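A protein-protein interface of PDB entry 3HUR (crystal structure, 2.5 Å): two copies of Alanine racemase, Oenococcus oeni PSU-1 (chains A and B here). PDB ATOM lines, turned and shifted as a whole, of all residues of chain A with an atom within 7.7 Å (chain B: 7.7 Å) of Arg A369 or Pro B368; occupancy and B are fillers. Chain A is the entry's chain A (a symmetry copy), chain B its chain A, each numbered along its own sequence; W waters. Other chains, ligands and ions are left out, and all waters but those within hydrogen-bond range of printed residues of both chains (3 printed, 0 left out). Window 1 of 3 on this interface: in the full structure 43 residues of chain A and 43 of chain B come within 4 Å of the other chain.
The side-chain amide nitrogen (ND2) of Asn A291 sits close to the side-chain carboxylate (OE2) of Glu B350, 2.3 Å away.
O of Ile B370 sits at hydrogen-bond distance from NH1 of Arg B372.
The backbone NH of Val B348 sits at hydrogen-bond distance from the backbone carbonyl oxygen of Gln B363.
The guanidinium group of Arg A372 lies within hydrogen-bond range of the backbone carbonyl oxygen of Ile A370 (3.1 Å).
The backbone carbonyl oxygen (O) of Glu B350 lies within hydrogen-bond range of the backbone NH (N) of Glu B361 (2.8 Å).
The side-chain hydroxyl (OG1) of Thr B364 lies within hydrogen-bond range of the backbone NH (N) of Leu B366.
OG1 of Thr A364 is in hydrogen-bond range of N of Leu A366 (3.1 Å).
Thr A10 touches Glu B361.
CB of Arg B369 touches OE1 of Gln A363, at 3.6 Å.
Ile B370 touches Gln A363.
Thr A364 touches Arg B369.
Pro A368 touches Arg B369 (CB to CG, 3.6 Å).
Arg A369 touches Gln B363 (CB to OE1, 3.6 Å).
CD of Arg A369 touches O of Thr B364, 3.2 Å away.
Pro B368 touches Arg A369.
Ile A370 touches Gln B363.
Printed residues of chain B within 4 Å of Asn A291: Glu B350.
Of the printed residues of chain B, Gln A363 touches Arg B369 (3.6 Å) and Ile B370 (3.8 Å).
Of chain B, only Gln B363 (3.6 Å), Thr B364 (3.2 Å) and Pro B368 (3.6 Å) come within 4 Å of Arg A369.
Gly B45 touches none of the printed residues of chain A.
Printed residues of chain A within 4 Å of Arg B369: Gln A363 (3.6 Å), Thr A364 (3.2 Å) and Pro A368 (3.6 Å).
The nearest residue of chain B that does not touch Arg A369 is Val B348 (4.5 Å).
Of the 19 printed residues of chain B, 7 touch a printed residue of chain A.
Printed residues of chain B that touch a printed residue of chain A: Glu B350, Glu B361, Gln B363, Thr B364, Pro B368, Arg B369 and Ile B370.
Hydrophobic or aromatic side chains of chain B within 4 Å of the printed part of chain A: Pro B368 and Ile B370.
Of the 17 printed residues of chain A, 7 touch a printed residue of chain B.
Among the printed residues, 10 pairs touch across the chains.
Gln A363 touches Arg B369, and with the chains exchanged Arg A369 touches Gln B363.
Gln A363 touches Ile B370, and with the chains exchanged Ile A370 touches Gln B363.
Thr A364 touches Arg B369, and with the chains exchanged Arg A369 touches Thr B364.
Pro A368 touches Arg B369, and with the chains exchanged Arg A369 touches Pro B368.
Of the 10 pairs that touch across the chains among the printed residues, 8 have their exchanged pair printed and touching as well.
Water W1 lies within hydrogen-bond range of OD1 of Asp A292 (2.5 Å), NE2 of Gln B363 (3.0 Å) and OE1 of Glu B350 (3.5 Å).
Water W2 lies within hydrogen-bond range of the backbone NH of Thr B364 (2.8 Å) and the backbone carbonyl oxygen of Arg A369 (2.9 Å).
Water W3 bridges the backbone NH (N) of Thr A364 (2.8 Å) and the backbone carbonyl oxygen (O) of Arg B369 (2.9 Å).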
ATOM      1  N   ARG A   8      20.469 -11.198 -14.771  1.00  0.00           N
ATOM      2  CA  ARG A   8      19.108 -11.760 -14.552  1.00  0.00           C
ATOM      3  C   ARG A   8      18.629 -11.456 -13.103  1.00  0.00           C
ATOM      4  O   ARG A   8      18.661 -12.337 -12.233  1.00  0.00           O
ATOM      5  CB  ARG A   8      19.176 -13.286 -14.782  1.00  0.00           C
ATOM      6  CG  ARG A   8      17.914 -14.084 -14.477  1.00  0.00           C
ATOM      7  CD  ARG A   8      17.161 -14.455 -15.710  1.00  0.00           C
ATOM      8  NE  ARG A   8      17.934 -15.224 -16.694  1.00  0.00           N
ATOM      9  CZ  ARG A   8      17.848 -15.039 -18.014  1.00  0.00           C
ATOM     10  NH1 ARG A   8      18.585 -15.776 -18.845  1.00  0.00           N
ATOM     11  NH2 ARG A   8      17.035 -14.103 -18.523  1.00  0.00           N
ATOM     12  N   THR A  10      15.762 -10.435 -11.854  1.00  0.00           N
ATOM     13  CA  THR A  10      14.509 -10.952 -11.418  1.00  0.00           C
ATOM     14  C   THR A  10      14.087 -12.067 -12.359  1.00  0.00           C
ATOM     15  O   THR A  10      14.528 -12.110 -13.493  1.00  0.00           O
ATOM     16  CB  THR A  10      13.460  -9.848 -11.419  1.00  0.00           C
ATOM     17  OG1 THR A  10      13.338  -9.286 -12.743  1.00  0.00           O
ATOM     18  CG2 THR A  10      13.795  -8.784 -10.434  1.00  0.00           C
ATOM     19  N   VAL A  12      10.759 -15.495 -12.862  1.00  0.00           N
ATOM     20  CA  VAL A  12       9.623 -16.312 -12.383  1.00  0.00           C
ATOM     21  C   VAL A  12      10.117 -17.704 -12.301  1.00  0.00           C
ATOM     22  O   VAL A  12      10.536 -18.263 -13.296  1.00  0.00           O
ATOM     23  CB  VAL A  12       8.427 -16.396 -13.348  1.00  0.00           C
ATOM     24  CG1 VAL A  12       7.324 -17.309 -12.746  1.00  0.00           C
ATOM     25  CG2 VAL A  12       7.883 -15.025 -13.643  1.00  0.00           C
ATOM     26  N   TYR A 290       9.814   0.245  -8.684  1.00  0.00           N
ATOM     27  CA  TYR A 290       8.569   0.607  -9.350  1.00  0.00           C
ATOM     28  C   TYR A 290       8.613   0.556 -10.850  1.00  0.00           C
ATOM     29  O   TYR A 290       7.583   0.760 -11.452  1.00  0.00           O
ATOM     30  CB  TYR A 290       8.080   1.986  -8.893  1.00  0.00           C
ATOM     31  CG  TYR A 290       7.655   1.990  -7.444  1.00  0.00           C
ATOM     32  CD1 TYR A 290       6.502   1.329  -7.036  1.00  0.00           C
ATOM     33  CD2 TYR A 290       8.394   2.670  -6.481  1.00  0.00           C
ATOM     34  CE1 TYR A 290       6.121   1.323  -5.694  1.00  0.00           C
ATOM     35  CE2 TYR A 290       8.015   2.673  -5.146  1.00  0.00           C
ATOM     36  CZ  TYR A 290       6.889   2.006  -4.752  1.00  0.00           C
ATOM     37  OH  TYR A 290       6.526   2.042  -3.406  1.00  0.00           O
ATOM     38  N   ASN A 291       9.791   0.358 -11.452  1.00  0.00           N
ATOM     39  CA  ASN A 291       9.899   0.093 -12.894  1.00  0.00           C
ATOM     40  C   ASN A 291       9.206  -1.188 -13.236  1.00  0.00           C
ATOM     41  O   ASN A 291       8.917  -1.411 -14.405  1.00  0.00           O
ATOM     42  CB  ASN A 291      11.340  -0.169 -13.322  1.00  0.00           C
ATOM     43  CG  ASN A 291      11.979   0.996 -13.975  1.00  0.00           C
ATOM     44  OD1 ASN A 291      11.296   1.953 -14.342  1.00  0.00           O
ATOM     45  ND2 ASN A 291      13.320   0.934 -14.140  1.00  0.00           N
ATOM     46  N   ASP A 292       9.049  -2.059 -12.235  1.00  0.00           N
ATOM     47  CA  ASP A 292       8.562  -3.400 -12.456  1.00  0.00           C
ATOM     48  C   ASP A 292       7.081  -3.450 -12.184  1.00  0.00           C
ATOM     49  O   ASP A 292       6.638  -3.469 -11.028  1.00  0.00           O
ATOM     50  CB  ASP A 292       9.309  -4.395 -11.565  1.00  0.00           C
ATOM     51  CG  ASP A 292      10.814  -4.450 -11.886  1.00  0.00           C
ATOM     52  OD1 ASP A 292      11.153  -4.837 -13.007  1.00  0.00           O
ATOM     53  OD2 ASP A 292      11.653  -4.123 -11.015  1.00  0.00           O
ATOM     54  N   GLY A 293       6.320  -3.471 -13.264  1.00  0.00           N
ATOM     55  CA  GLY A 293       4.895  -3.453 -13.188  1.00  0.00           C
ATOM     56  C   GLY A 293       4.351  -4.613 -12.421  1.00  0.00           C
ATOM     57  O   GLY A 293       3.359  -4.465 -11.770  1.00  0.00           O
ATOM     58  N   TRP A 294       4.990  -5.764 -12.471  1.00  0.00           N
ATOM     59  CA  TRP A 294       4.573  -6.845 -11.621  1.00  0.00           C
ATOM     60  C   TRP A 294       4.630  -6.516 -10.133  1.00  0.00           C
ATOM     61  O   TRP A 294       4.052  -7.233  -9.311  1.00  0.00           O
ATOM     62  CB  TRP A 294       5.426  -8.108 -11.882  1.00  0.00           C
ATOM     63  CG  TRP A 294       6.937  -7.967 -11.692  1.00  0.00           C
ATOM     64  CD1 TRP A 294       7.875  -7.750 -12.685  1.00  0.00           C
ATOM     65  CD2 TRP A 294       7.675  -8.038 -10.463  1.00  0.00           C
ATOM     66  NE1 TRP A 294       9.113  -7.705 -12.147  1.00  0.00           N
ATOM     67  CE2 TRP A 294       9.030  -7.884 -10.787  1.00  0.00           C
ATOM     68  CE3 TRP A 294       7.324  -8.243  -9.141  1.00  0.00           C
ATOM     69  CZ2 TRP A 294      10.039  -7.887  -9.826  1.00  0.00           C
ATOM     70  CZ3 TRP A 294       8.332  -8.257  -8.157  1.00  0.00           C
ATOM     71  CH2 TRP A 294       9.675  -8.068  -8.511  1.00  0.00           C
ATOM     72  N   GLN A 363      -4.054 -14.421 -22.125  1.00  0.00           N
ATOM     73  CA  GLN A 363      -2.773 -13.752 -22.002  1.00  0.00           C
ATOM     74  C   GLN A 363      -2.274 -13.742 -20.575  1.00  0.00           C
ATOM     75  O   GLN A 363      -3.073 -13.680 -19.665  1.00  0.00           O
ATOM     76  CB  GLN A 363      -2.886 -12.315 -22.465  1.00  0.00           C
ATOM     77  CG  GLN A 363      -2.822 -12.149 -23.932  1.00  0.00           C
ATOM     78  CD  GLN A 363      -2.891 -10.685 -24.351  1.00  0.00           C
ATOM     79  OE1 GLN A 363      -1.987 -10.174 -25.018  1.00  0.00           O
ATOM     80  NE2 GLN A 363      -3.942 -10.012 -23.958  1.00  0.00           N
ATOM     81  N   THR A 364      -0.949 -13.792 -20.395  1.00  0.00           N
ATOM     82  CA  THR A 364      -0.353 -13.728 -19.061  1.00  0.00           C
ATOM     83  C   THR A 364      -0.519 -12.338 -18.467  1.00  0.00           C
ATOM     84  O   THR A 364      -0.655 -11.344 -19.194  1.00  0.00           O
ATOM     85  CB  THR A 364       1.156 -14.072 -19.032  1.00  0.00           C
ATOM     86  OG1 THR A 364       1.575 -14.186 -17.661  1.00  0.00           O
ATOM     87  CG2 THR A 364       1.965 -12.999 -19.690  1.00  0.00           C
ATOM     88  N   LEU A 366       1.340 -12.156 -15.395  1.00  0.00           N
ATOM     89  CA  LEU A 366       2.421 -12.310 -14.439  1.00  0.00           C
ATOM     90  C   LEU A 366       3.776 -11.958 -15.110  1.00  0.00           C
ATOM     91  O   LEU A 366       4.361 -12.787 -15.797  1.00  0.00           O
ATOM     92  CB  LEU A 366       2.433 -13.722 -13.864  1.00  0.00           C
ATOM     93  CG  LEU A 366       3.485 -13.977 -12.784  1.00  0.00           C
ATOM     94  CD1 LEU A 366       3.174 -13.186 -11.522  1.00  0.00           C
ATOM     95  CD2 LEU A 366       3.691 -15.459 -12.429  1.00  0.00           C
ATOM     96  N   ALA A 367       4.240 -10.718 -14.909  1.00  0.00           N
ATOM     97  CA  ALA A 367       5.640 -10.298 -15.174  1.00  0.00           C
ATOM     98  C   ALA A 367       6.076 -10.789 -16.512  1.00  0.00           C
ATOM     99  O   ALA A 367       7.033 -11.521 -16.628  1.00  0.00           O
ATOM    100  CB  ALA A 367       6.573 -10.808 -14.112  1.00  0.00           C
ATOM    101  N   PRO A 368       5.371 -10.364 -17.533  1.00  0.00           N
ATOM    102  CA  PRO A 368       5.578 -10.870 -18.878  1.00  0.00           C
ATOM    103  C   PRO A 368       6.968 -10.622 -19.466  1.00  0.00           C
ATOM    104  O   PRO A 368       7.362 -11.332 -20.422  1.00  0.00           O
ATOM    105  CB  PRO A 368       4.515 -10.169 -19.711  1.00  0.00           C
ATOM    106  CG  PRO A 368       4.121  -8.982 -18.949  1.00  0.00           C
ATOM    107  CD  PRO A 368       4.509  -9.173 -17.484  1.00  0.00           C
ATOM    108  N   ARG A 369       7.721  -9.686 -18.902  1.00  0.00           N
ATOM    109  CA  ARG A 369       8.975  -9.315 -19.493  1.00  0.00           C
ATOM    110  C   ARG A 369      10.159 -10.006 -18.891  1.00  0.00           C
ATOM    111  O   ARG A 369      11.262  -9.803 -19.389  1.00  0.00           O
ATOM    112  CB  ARG A 369       9.147  -7.803 -19.445  1.00  0.00           C
ATOM    113  CG  ARG A 369       8.229  -7.105 -20.480  1.00  0.00           C
ATOM    114  CD  ARG A 369       8.288  -5.599 -20.426  1.00  0.00           C
ATOM    115  NE  ARG A 369       8.148  -5.085 -19.078  1.00  0.00           N
ATOM    116  CZ  ARG A 369       8.784  -4.011 -18.603  1.00  0.00           C
ATOM    117  NH1 ARG A 369       9.620  -3.307 -19.373  1.00  0.00           N
ATOM    118  NH2 ARG A 369       8.581  -3.632 -17.340  1.00  0.00           N
ATOM    119  N   ILE A 370       9.955 -10.852 -17.863  1.00  0.00           N
ATOM    120  CA  ILE A 370      11.056 -11.610 -17.239  1.00  0.00           C
ATOM    121  C   ILE A 370      11.023 -13.135 -17.556  1.00  0.00           C
ATOM    122  O   ILE A 370      10.006 -13.686 -17.920  1.00  0.00           O
ATOM    123  CB  ILE A 370      11.155 -11.354 -15.695  1.00  0.00           C
ATOM    124  CG1 ILE A 370      10.103 -12.116 -14.913  1.00  0.00           C
ATOM    125  CG2 ILE A 370      11.021  -9.894 -15.377  1.00  0.00           C
ATOM    126  CD1 ILE A 370      10.107 -11.769 -13.395  1.00  0.00           C
ATOM    127  N   LYS A 371      12.161 -13.796 -17.412  1.00  0.00           N
ATOM    128  CA  LYS A 371      12.341 -15.127 -17.890  1.00  0.00           C
ATOM    129  C   LYS A 371      11.739 -16.112 -16.913  1.00  0.00           C
ATOM    130  O   LYS A 371      11.714 -15.874 -15.705  1.00  0.00           O
ATOM    131  CB  LYS A 371      13.834 -15.415 -18.047  1.00  0.00           C
ATOM    132  CG  LYS A 371      14.160 -16.830 -18.530  1.00  0.00           C
ATOM    133  CD  LYS A 371      14.967 -16.811 -19.804  1.00  0.00           C
ATOM    134  CE  LYS A 371      15.386 -18.220 -20.256  1.00  0.00           C
ATOM    135  NZ  LYS A 371      15.796 -18.138 -21.697  1.00  0.00           N
ATOM    136  N   ARG A 372      11.298 -17.235 -17.444  1.00  0.00           N
ATOM    137  CA  ARG A 372      10.847 -18.322 -16.640  1.00  0.00           C
ATOM    138  C   ARG A 372      12.034 -19.248 -16.378  1.00  0.00           C
ATOM    139  O   ARG A 372      12.668 -19.681 -17.320  1.00  0.00           O
ATOM    140  CB  ARG A 372       9.715 -19.059 -17.362  1.00  0.00           C
ATOM    141  CG  ARG A 372       8.351 -18.474 -17.128  1.00  0.00           C
ATOM    142  CD  ARG A 372       8.225 -17.029 -17.488  1.00  0.00           C
ATOM    143  NE  ARG A 372       6.830 -16.625 -17.356  1.00  0.00           N
ATOM    144  CZ  ARG A 372       6.367 -15.394 -17.107  1.00  0.00           C
ATOM    145  NH1 ARG A 372       7.152 -14.349 -16.991  1.00  0.00           N
ATOM    146  NH2 ARG A 372       5.064 -15.216 -16.995  1.00  0.00           N
ATOM    147  N   VAL B  12       3.522 -10.807 -33.189  1.00  0.00           N
ATOM    148  CA  VAL B  12       4.722 -10.128 -33.724  1.00  0.00           C
ATOM    149  C   VAL B  12       5.310 -11.047 -34.724  1.00  0.00           C
ATOM    150  O   VAL B  12       5.672 -12.159 -34.392  1.00  0.00           O
ATOM    151  CB  VAL B  12       5.856  -9.911 -32.705  1.00  0.00           C
ATOM    152  CG1 VAL B  12       7.067  -9.226 -33.398  1.00  0.00           C
ATOM    153  CG2 VAL B  12       5.375  -9.090 -31.539  1.00  0.00           C
ATOM    154  N   ALA B  41      18.685 -10.607 -24.179  1.00  0.00           N
ATOM    155  CA  ALA B  41      17.251 -10.476 -23.893  1.00  0.00           C
ATOM    156  C   ALA B  41      16.413 -11.265 -24.897  1.00  0.00           C
ATOM    157  O   ALA B  41      15.529 -10.719 -25.530  1.00  0.00           O
ATOM    158  CB  ALA B  41      16.828  -8.976 -23.918  1.00  0.00           C
ATOM    159  N   GLY B  45      14.133  -9.561 -27.503  1.00  0.00           N
ATOM    160  CA  GLY B  45      12.721  -9.874 -27.465  1.00  0.00           C
ATOM    161  C   GLY B  45      12.095 -10.401 -28.741  1.00  0.00           C
ATOM    162  O   GLY B  45      10.879 -10.382 -28.855  1.00  0.00           O
ATOM    163  N   GLY B 293      -1.514  -2.577 -24.743  1.00  0.00           N
ATOM    164  CA  GLY B 293      -0.575  -1.556 -24.406  1.00  0.00           C
ATOM    165  C   GLY B 293       0.377  -1.269 -25.520  1.00  0.00           C
ATOM    166  O   GLY B 293       0.778  -0.153 -25.668  1.00  0.00           O
ATOM    167  N   TRP B 294       0.737  -2.254 -26.319  1.00  0.00           N
ATOM    168  CA  TRP B 294       1.528  -1.969 -27.484  1.00  0.00           C
ATOM    169  C   TRP B 294       0.863  -1.001 -28.458  1.00  0.00           C
ATOM    170  O   TRP B 294       1.522  -0.458 -29.349  1.00  0.00           O
ATOM    171  CB  TRP B 294       1.874  -3.271 -28.243  1.00  0.00           C
ATOM    172  CG  TRP B 294       0.697  -4.125 -28.716  1.00  0.00           C
ATOM    173  CD1 TRP B 294       0.178  -5.237 -28.078  1.00  0.00           C
ATOM    174  CD2 TRP B 294      -0.091  -3.949 -29.903  1.00  0.00           C
ATOM    175  NE1 TRP B 294      -0.843  -5.748 -28.801  1.00  0.00           N
ATOM    176  CE2 TRP B 294      -1.032  -4.987 -29.931  1.00  0.00           C
ATOM    177  CE3 TRP B 294      -0.069  -3.041 -30.945  1.00  0.00           C
ATOM    178  CZ2 TRP B 294      -1.977  -5.120 -30.945  1.00  0.00           C
ATOM    179  CZ3 TRP B 294      -1.012  -3.165 -31.985  1.00  0.00           C
ATOM    180  CH2 TRP B 294      -1.960  -4.196 -31.965  1.00  0.00           C
ATOM    181  N   VAL B 348      14.695  -1.862 -23.720  1.00  0.00           N
ATOM    182  CA  VAL B 348      15.157  -0.866 -22.787  1.00  0.00           C
ATOM    183  C   VAL B 348      16.215  -1.564 -21.926  1.00  0.00           C
ATOM    184  O   VAL B 348      16.059  -2.714 -21.576  1.00  0.00           O
ATOM    185  CB  VAL B 348      13.998  -0.270 -21.887  1.00  0.00           C
ATOM    186  CG1 VAL B 348      13.246  -1.383 -21.105  1.00  0.00           C
ATOM    187  CG2 VAL B 348      14.509   0.796 -20.870  1.00  0.00           C
ATOM    188  N   GLU B 350      18.729  -1.142 -18.318  1.00  0.00           N
ATOM    189  CA  GLU B 350      18.806  -0.545 -16.992  1.00  0.00           C
ATOM    190  C   GLU B 350      20.107  -1.097 -16.390  1.00  0.00           C
ATOM    191  O   GLU B 350      20.278  -2.301 -16.359  1.00  0.00           O
ATOM    192  CB  GLU B 350      17.560  -1.031 -16.215  1.00  0.00           C
ATOM    193  CG  GLU B 350      17.368  -0.654 -14.695  1.00  0.00           C
ATOM    194  CD  GLU B 350      15.894  -0.987 -14.161  1.00  0.00           C
ATOM    195  OE1 GLU B 350      15.349  -2.096 -14.436  1.00  0.00           O
ATOM    196  OE2 GLU B 350      15.257  -0.128 -13.474  1.00  0.00           O
ATOM    197  N   GLU B 361      20.356  -5.086 -16.849  1.00  0.00           N
ATOM    198  CA  GLU B 361      19.092  -5.712 -17.315  1.00  0.00           C
ATOM    199  C   GLU B 361      18.524  -5.176 -18.627  1.00  0.00           C
ATOM    200  O   GLU B 361      18.109  -4.045 -18.672  1.00  0.00           O
ATOM    201  CB  GLU B 361      18.024  -5.476 -16.262  1.00  0.00           C
ATOM    202  CG  GLU B 361      16.763  -6.339 -16.484  1.00  0.00           C
ATOM    203  CD  GLU B 361      15.673  -6.087 -15.460  1.00  0.00           C
ATOM    204  OE1 GLU B 361      15.641  -4.948 -14.898  1.00  0.00           O
ATOM    205  OE2 GLU B 361      14.847  -7.034 -15.239  1.00  0.00           O
ATOM    206  N   ILE B 362      18.463  -5.984 -19.678  1.00  0.00           N
ATOM    207  CA  ILE B 362      17.765  -5.577 -20.887  1.00  0.00           C
ATOM    208  C   ILE B 362      16.428  -6.299 -20.934  1.00  0.00           C
ATOM    209  O   ILE B 362      16.349  -7.459 -20.525  1.00  0.00           O
ATOM    210  CB  ILE B 362      18.569  -5.858 -22.151  1.00  0.00           C
ATOM    211  CG1 ILE B 362      19.916  -5.150 -22.060  1.00  0.00           C
ATOM    212  CG2 ILE B 362      17.857  -5.317 -23.330  1.00  0.00           C
ATOM    213  CD1 ILE B 362      20.816  -5.239 -23.327  1.00  0.00           C
ATOM    214  N   GLN B 363      15.396  -5.598 -21.431  1.00  0.00           N
ATOM    215  CA  GLN B 363      14.034  -6.094 -21.486  1.00  0.00           C
ATOM    216  C   GLN B 363      13.302  -5.606 -22.715  1.00  0.00           C
ATOM    217  O   GLN B 363      13.559  -4.510 -23.164  1.00  0.00           O
ATOM    218  CB  GLN B 363      13.260  -5.634 -20.269  1.00  0.00           C
ATOM    219  CG  GLN B 363      13.499  -6.449 -19.060  1.00  0.00           C
ATOM    220  CD  GLN B 363      12.664  -5.981 -17.873  1.00  0.00           C
ATOM    221  OE1 GLN B 363      11.881  -6.749 -17.308  1.00  0.00           O
ATOM    222  NE2 GLN B 363      12.818  -4.735 -17.504  1.00  0.00           N
ATOM    223  N   THR B 364      12.384  -6.426 -23.240  1.00  0.00           N
ATOM    224  CA  THR B 364      11.574  -6.031 -24.392  1.00  0.00           C
ATOM    225  C   THR B 364      10.582  -4.947 -24.002  1.00  0.00           C
ATOM    226  O   THR B 364      10.195  -4.823 -22.832  1.00  0.00           O
ATOM    227  CB  THR B 364      10.770  -7.196 -25.020  1.00  0.00           C
ATOM    228  OG1 THR B 364      10.192  -6.741 -26.255  1.00  0.00           O
ATOM    229  CG2 THR B 364       9.667  -7.640 -24.112  1.00  0.00           C
ATOM    230  N   THR B 365      10.275  -4.111 -24.975  1.00  0.00           N
ATOM    231  CA  THR B 365       9.264  -3.076 -24.861  1.00  0.00           C
ATOM    232  C   THR B 365       8.296  -3.228 -26.044  1.00  0.00           C
ATOM    233  O   THR B 365       7.552  -2.291 -26.333  1.00  0.00           O
ATOM    234  CB  THR B 365       9.893  -1.623 -24.936  1.00  0.00           C
ATOM    235  OG1 THR B 365      10.513  -1.466 -26.222  1.00  0.00           O
ATOM    236  CG2 THR B 365      10.906  -1.387 -23.832  1.00  0.00           C
ATOM    237  N   LEU B 366       8.361  -4.354 -26.768  1.00  0.00           N
ATOM    238  CA  LEU B 366       7.470  -4.608 -27.885  1.00  0.00           C
ATOM    239  C   LEU B 366       6.487  -5.756 -27.531  1.00  0.00           C
ATOM    240  O   LEU B 366       6.838  -6.926 -27.638  1.00  0.00           O
ATOM    241  CB  LEU B 366       8.266  -4.923 -29.146  1.00  0.00           C
ATOM    242  CG  LEU B 366       7.431  -5.131 -30.410  1.00  0.00           C
ATOM    243  CD1 LEU B 366       6.765  -3.833 -30.842  1.00  0.00           C
ATOM    244  CD2 LEU B 366       8.201  -5.737 -31.595  1.00  0.00           C
ATOM    245  N   ALA B 367       5.274  -5.394 -27.096  1.00  0.00           N
ATOM    246  CA  ALA B 367       4.105  -6.308 -27.027  1.00  0.00           C
ATOM    247  C   ALA B 367       4.503  -7.599 -26.396  1.00  0.00           C
ATOM    248  O   ALA B 367       4.379  -8.648 -26.988  1.00  0.00           O
ATOM    249  CB  ALA B 367       3.529  -6.560 -28.391  1.00  0.00           C
ATOM    250  N   PRO B 368       4.971  -7.517 -25.173  1.00  0.00           N
ATOM    251  CA  PRO B 368       5.536  -8.663 -24.485  1.00  0.00           C
ATOM    252  C   PRO B 368       4.578  -9.835 -24.264  1.00  0.00           C
ATOM    253  O   PRO B 368       5.050 -10.976 -24.043  1.00  0.00           O
ATOM    254  CB  PRO B 368       6.010  -8.104 -23.151  1.00  0.00           C
ATOM    255  CG  PRO B 368       5.266  -6.858 -22.947  1.00  0.00           C
ATOM    256  CD  PRO B 368       4.736  -6.363 -24.291  1.00  0.00           C
ATOM    257  N   ARG B 369       3.277  -9.597 -24.361  1.00  0.00           N
ATOM    258  CA  ARG B 369       2.329 -10.622 -24.030  1.00  0.00           C
ATOM    259  C   ARG B 369       1.828 -11.393 -25.213  1.00  0.00           C
ATOM    260  O   ARG B 369       1.072 -12.338 -25.010  1.00  0.00           O
ATOM    261  CB  ARG B 369       1.171 -10.027 -23.241  1.00  0.00           C
ATOM    262  CG  ARG B 369       1.601  -9.684 -21.793  1.00  0.00           C
ATOM    263  CD  ARG B 369       0.523  -9.011 -20.981  1.00  0.00           C
ATOM    264  NE  ARG B 369      -0.094  -7.905 -21.686  1.00  0.00           N
ATOM    265  CZ  ARG B 369      -1.386  -7.577 -21.604  1.00  0.00           C
ATOM    266  NH1 ARG B 369      -2.228  -8.270 -20.830  1.00  0.00           N
ATOM    267  NH2 ARG B 369      -1.847  -6.538 -22.304  1.00  0.00           N
ATOM    268  N   ILE B 370       2.265 -11.043 -26.438  1.00  0.00           N
ATOM    269  CA  ILE B 370       1.861 -11.775 -27.654  1.00  0.00           C
ATOM    270  C   ILE B 370       3.006 -12.626 -28.281  1.00  0.00           C
ATOM    271  O   ILE B 370       4.171 -12.394 -28.044  1.00  0.00           O
ATOM    272  CB  ILE B 370       1.202 -10.836 -28.724  1.00  0.00           C
ATOM    273  CG1 ILE B 370       2.227 -10.015 -29.481  1.00  0.00           C
ATOM    274  CG2 ILE B 370       0.215  -9.900 -28.089  1.00  0.00           C
ATOM    275  CD1 ILE B 370       1.578  -8.984 -30.453  1.00  0.00           C
ATOM    276  N   LYS B 371       2.639 -13.616 -29.081  1.00  0.00           N
ATOM    277  CA  LYS B 371       3.550 -14.617 -29.528  1.00  0.00           C
ATOM    278  C   LYS B 371       4.367 -14.090 -30.688  1.00  0.00           C
ATOM    279  O   LYS B 371       3.896 -13.268 -31.474  1.00  0.00           O
ATOM    280  CB  LYS B 371       2.770 -15.853 -29.977  1.00  0.00           C
ATOM    281  CG  LYS B 371       3.640 -16.993 -30.509  1.00  0.00           C
ATOM    282  CD  LYS B 371       3.420 -18.268 -29.734  1.00  0.00           C
ATOM    283  CE  LYS B 371       4.214 -19.453 -30.312  1.00  0.00           C
ATOM    284  NZ  LYS B 371       4.268 -20.525 -29.264  1.00  0.00           N
ATOM    285  N   ARG B 372       5.574 -14.605 -30.807  1.00  0.00           N
ATOM    286  CA  ARG B 372       6.403 -14.328 -31.932  1.00  0.00           C
ATOM    287  C   ARG B 372       6.152 -15.402 -32.989  1.00  0.00           C
ATOM    288  O   ARG B 372       6.268 -16.573 -32.684  1.00  0.00           O
ATOM    289  CB  ARG B 372       7.872 -14.308 -31.496  1.00  0.00           C
ATOM    290  CG  ARG B 372       8.341 -12.981 -30.970  1.00  0.00           C
ATOM    291  CD  ARG B 372       7.542 -12.449 -29.825  1.00  0.00           C
ATOM    292  NE  ARG B 372       8.183 -11.241 -29.317  1.00  0.00           N
ATOM    293  CZ  ARG B 372       7.595 -10.226 -28.673  1.00  0.00           C
ATOM    294  NH1 ARG B 372       6.317 -10.219 -28.372  1.00  0.00           N
ATOM    295  NH2 ARG B 372       8.332  -9.195 -28.305  1.00  0.00           N
HETATM  296  O   HOH W   1      12.192  -3.485 -14.897  1.00  0.00           O
HETATM  297  O   HOH W   2      12.361  -8.903 -21.916  1.00  0.00           O
HETATM  298  O   HOH W   3       0.393 -14.135 -22.839  1.00  0.00           O
